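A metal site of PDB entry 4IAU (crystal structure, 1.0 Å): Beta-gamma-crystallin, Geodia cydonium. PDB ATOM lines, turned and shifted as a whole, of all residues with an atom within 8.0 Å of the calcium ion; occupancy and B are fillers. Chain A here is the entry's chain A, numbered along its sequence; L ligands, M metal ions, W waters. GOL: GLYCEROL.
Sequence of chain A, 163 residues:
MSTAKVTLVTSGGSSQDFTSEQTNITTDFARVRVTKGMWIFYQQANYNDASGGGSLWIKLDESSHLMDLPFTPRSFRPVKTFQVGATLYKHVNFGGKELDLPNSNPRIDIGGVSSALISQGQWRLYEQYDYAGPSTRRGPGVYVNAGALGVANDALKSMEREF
The side-chain carboxylate of Asp 154 is in hydrogen-bond range of the side-chain amide nitrogen of Asn 153, 3.4 Å away.
The backbone NH (N) of Ala 146 is in hydrogen-bond range of the backbone carbonyl oxygen (O) of Ser 114.
N of Ser 114 sits at hydrogen-bond distance from O of Tyr 89 (2.9 Å).
The backbone NH (N) of Asp 154 sits at hydrogen-bond distance from the backbone carbonyl oxygen (O) of Val 113.
N of Lys 90 is in hydrogen-bond range of O of Gly 95 (3.4 Å).
OD1 of Asn 153 lies close to OG of Ser 114 (2.7 Å).
The calcium ion is bound by O of Lys 90 (2.3 Å), water W1 (2.3 Å), OG of Ser 114 (2.4 Å), OD1 of Asp 154 (2.4 Å), O2 of the ligand (2.4 Å), O of Gly 112 (2.5 Å) and O1 of the ligand (2.5 Å).
Four residues have an atom within 4 Å of the calcium ion: Lys 90, Gly 112, Ser 114 and Asp 154.
The nearest printed residue that does not touch the calcium ion is Val 113 (4.2 Å).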
ATOM      1  N   GLY A  52       9.235   2.660   0.271  1.00  0.00           N
ATOM      2  CA  GLY A  52       9.680   3.111  -1.034  1.00  0.00           C
ATOM      3  C   GLY A  52      10.147   4.552  -1.005  1.00  0.00           C
ATOM      4  O   GLY A  52       9.947   5.318  -1.943  1.00  0.00           O
ATOM      5  N   TYR A  89      20.020   6.294  -6.035  1.00  0.00           N
ATOM      6  CA  TYR A  89      19.198   5.590  -5.054  1.00  0.00           C
ATOM      7  C   TYR A  89      17.971   4.998  -5.716  1.00  0.00           C
ATOM      8  O   TYR A  89      17.377   5.582  -6.650  1.00  0.00           O
ATOM      9  CB  TYR A  89      18.768   6.566  -3.953  1.00  0.00           C
ATOM     10  CG  TYR A  89      19.912   7.172  -3.222  1.00  0.00           C
ATOM     11  CD1 TYR A  89      20.437   6.572  -2.089  1.00  0.00           C
ATOM     12  CD2 TYR A  89      20.488   8.389  -3.628  1.00  0.00           C
ATOM     13  CE1 TYR A  89      21.503   7.148  -1.381  1.00  0.00           C
ATOM     14  CE2 TYR A  89      21.540   8.947  -2.949  1.00  0.00           C
ATOM     15  CZ  TYR A  89      22.058   8.320  -1.817  1.00  0.00           C
ATOM     16  OH  TYR A  89      23.119   8.935  -1.177  1.00  0.00           O
ATOM     17  N   LYS A  90      17.588   3.816  -5.238  1.00  0.00           N
ATOM     18  CA  LYS A  90      16.443   3.097  -5.804  1.00  0.00           C
ATOM     19  C   LYS A  90      15.139   3.823  -5.557  1.00  0.00           C
ATOM     20  O   LYS A  90      14.245   3.804  -6.398  1.00  0.00           O
ATOM     21  CB  LYS A  90      16.381   1.705  -5.200  1.00  0.00           C
ATOM     22  CG  LYS A  90      15.260   0.848  -5.755  1.00  0.00           C
ATOM     23  CD  LYS A  90      15.201  -0.531  -5.161  1.00  0.00           C
ATOM     24  CE  LYS A  90      14.135  -1.371  -5.782  1.00  0.00           C
ATOM     25  NZ  LYS A  90      14.050  -2.716  -5.103  1.00  0.00           N
ATOM     26  N   HIS A  91      14.954   4.469  -4.398  1.00  0.00           N
ATOM     27  CA  HIS A  91      13.692   5.116  -4.059  1.00  0.00           C
ATOM     28  C   HIS A  91      13.856   6.646  -4.113  1.00  0.00           C
ATOM     29  O   HIS A  91      14.969   7.172  -4.067  1.00  0.00           O
ATOM     30  CB  HIS A  91      13.209   4.696  -2.708  1.00  0.00           C
ATOM     31  CG  HIS A  91      13.000   3.256  -2.554  1.00  0.00           C
ATOM     32  ND1 HIS A  91      12.424   2.484  -3.526  1.00  0.00           N
ATOM     33  CD2 HIS A  91      13.332   2.454  -1.541  1.00  0.00           C
ATOM     34  CE1 HIS A  91      12.398   1.224  -3.091  1.00  0.00           C
ATOM     35  NE2 HIS A  91      12.926   1.163  -1.882  1.00  0.00           N
ATOM     36  N   VAL A  92      12.717   7.299  -4.230  1.00  0.00           N
ATOM     37  CA  VAL A  92      12.689   8.735  -4.026  1.00  0.00           C
ATOM     38  C   VAL A  92      13.271   9.059  -2.644  1.00  0.00           C
ATOM     39  O   VAL A  92      13.351   8.215  -1.747  1.00  0.00           O
ATOM     40  CB  VAL A  92      11.294   9.324  -4.169  1.00  0.00           C
ATOM     41  CG1 VAL A  92      10.747   9.153  -5.589  1.00  0.00           C
ATOM     42  CG2 VAL A  92      10.306   8.773  -3.123  1.00  0.00           C
ATOM     43  N   GLY A  95      16.090   6.846  -0.720  1.00  0.00           N
ATOM     44  CA  GLY A  95      15.849   5.609  -0.049  1.00  0.00           C
ATOM     45  C   GLY A  95      16.340   4.398  -0.805  1.00  0.00           C
ATOM     46  O   GLY A  95      16.602   4.426  -1.990  1.00  0.00           O
ATOM     47  N   ILE A 110      19.971  -1.152 -10.370  1.00  0.00           N
ATOM     48  CA  ILE A 110      19.649  -1.141  -8.924  1.00  0.00           C
ATOM     49  C   ILE A 110      18.152  -1.374  -8.693  1.00  0.00           C
ATOM     50  O   ILE A 110      17.705  -1.192  -7.549  1.00  0.00           O
ATOM     51  CB  ILE A 110      20.121   0.110  -8.200  1.00  0.00           C
ATOM     52  CG1 ILE A 110      19.429   1.367  -8.597  1.00  0.00           C
ATOM     53  CG2 ILE A 110      21.644   0.195  -8.320  1.00  0.00           C
ATOM     54  CD1 ILE A 110      19.817   2.601  -7.734  1.00  0.00           C
ATOM     55  N   GLY A 111      17.419  -1.804  -9.692  1.00  0.00           N
ATOM     56  CA  GLY A 111      15.986  -2.016  -9.528  1.00  0.00           C
ATOM     57  C   GLY A 111      15.204  -0.767  -9.805  1.00  0.00           C
ATOM     58  O   GLY A 111      14.009  -0.767  -9.465  1.00  0.00           O
ATOM     59  N   GLY A 112      15.793   0.196 -10.477  1.00  0.00           N
ATOM     60  CA  GLY A 112      15.071   1.376 -10.956  1.00  0.00           C
ATOM     61  C   GLY A 112      15.454   2.611 -10.141  1.00  0.00           C
ATOM     62  O   GLY A 112      15.059   2.787  -8.982  1.00  0.00           O
ATOM     63  N   VAL A 113      16.241   3.484 -10.748  1.00  0.00           N
ATOM     64  CA  VAL A 113      16.725   4.689 -10.067  1.00  0.00           C
ATOM     65  C   VAL A 113      15.584   5.680  -9.895  1.00  0.00           C
ATOM     66  O   VAL A 113      14.897   6.004 -10.863  1.00  0.00           O
ATOM     67  CB  VAL A 113      17.857   5.366 -10.861  1.00  0.00           C
ATOM     68  CG1 VAL A 113      18.262   6.679 -10.217  1.00  0.00           C
ATOM     69  CG2 VAL A 113      19.054   4.425 -10.986  1.00  0.00           C
ATOM     70  N   SER A 114      15.438   6.228  -8.685  1.00  0.00           N
ATOM     71  CA  SER A 114      14.454   7.241  -8.419  1.00  0.00           C
ATOM     72  C   SER A 114      14.959   8.528  -7.746  1.00  0.00           C
ATOM     73  O   SER A 114      14.163   9.459  -7.635  1.00  0.00           O
ATOM     74  CB  SER A 114      13.291   6.682  -7.585  1.00  0.00           C
ATOM     75  OG  SER A 114      12.675   5.585  -8.256  1.00  0.00           O
ATOM     76  N   SER A 115      16.204   8.624  -7.332  1.00  0.00           N
ATOM     77  CA  SER A 115      16.738   9.878  -6.825  1.00  0.00           C
ATOM     78  C   SER A 115      18.267   9.821  -6.893  1.00  0.00           C
ATOM     79  O   SER A 115      18.868   8.768  -7.140  1.00  0.00           O
ATOM     80  CB  SER A 115      16.251  10.204  -5.408  1.00  0.00           C
ATOM     81  OG  SER A 115      16.675   9.218  -4.464  1.00  0.00           O
ATOM     82  N   ALA A 146      13.119  11.387  -9.835  1.00  0.00           N
ATOM     83  CA  ALA A 146      13.711  11.192 -11.147  1.00  0.00           C
ATOM     84  C   ALA A 146      13.473  12.377 -12.081  1.00  0.00           C
ATOM     85  O   ALA A 146      14.331  12.746 -12.901  1.00  0.00           O
ATOM     86  CB  ALA A 146      13.163   9.923 -11.794  1.00  0.00           C
ATOM     87  N   ASN A 153      10.993   8.011 -14.190  1.00  0.00           N
ATOM     88  CA  ASN A 153      11.226   7.181 -13.027  1.00  0.00           C
ATOM     89  C   ASN A 153      11.656   5.782 -13.464  1.00  0.00           C
ATOM     90  O   ASN A 153      11.113   5.213 -14.419  1.00  0.00           O
ATOM     91  CB  ASN A 153       9.996   7.098 -12.133  1.00  0.00           C
ATOM     92  CG  ASN A 153      10.279   6.442 -10.816  1.00  0.00           C
ATOM     93  OD1 ASN A 153      11.277   6.831 -10.149  1.00  0.00           O
ATOM     94  ND2 ASN A 153       9.486   5.494 -10.403  1.00  0.00           N
ATOM     95  N   ASP A 154      12.621   5.207 -12.760  1.00  0.00           N
ATOM     96  CA  ASP A 154      13.118   3.860 -12.990  1.00  0.00           C
ATOM     97  C   ASP A 154      13.785   3.691 -14.349  1.00  0.00           C
ATOM     98  O   ASP A 154      14.078   2.560 -14.668  1.00  0.00           O
ATOM     99  CB  ASP A 154      12.021   2.819 -12.701  1.00  0.00           C
ATOM    100  CG  ASP A 154      11.608   2.847 -11.245  1.00  0.00           C
ATOM    101  OD1 ASP A 154      12.387   3.298 -10.401  1.00  0.00           O
ATOM    102  OD2 ASP A 154      10.494   2.314 -10.919  1.00  0.00           O
ATOM    103  N   ALA A 155      14.101   4.697 -15.060  1.00  0.00           N
ATOM    104  CA  ALA A 155      14.632   4.621 -16.410  1.00  0.00           C
ATOM    105  C   ALA A 155      16.105   4.881 -16.587  1.00  0.00           C
ATOM    106  O   ALA A 155      16.651   4.562 -17.658  1.00  0.00           O
ATOM    107  CB  ALA A 155      13.828   5.546 -17.325  1.00  0.00           C
HETATM  108  C1  GOL L   1       9.454   2.983  -7.320  1.00  0.00           C
HETATM  109  O1  GOL L   1      10.303   3.411  -8.408  1.00  0.00           O
HETATM  110  C2  GOL L   1      10.090   3.425  -5.997  1.00  0.00           C
HETATM  111  O2  GOL L   1      11.446   3.077  -6.020  1.00  0.00           O
HETATM  112  C3  GOL L   1       9.919   4.937  -5.855  1.00  0.00           C
HETATM  113  O3  GOL L   1      10.532   5.439  -4.668  1.00  0.00           O
HETATM  114 CA    CA M   1      12.778   3.228  -8.050  1.00  0.00          CA
HETATM  115  O   HOH W   1      12.475   0.902  -8.039  1.00  0.00           O
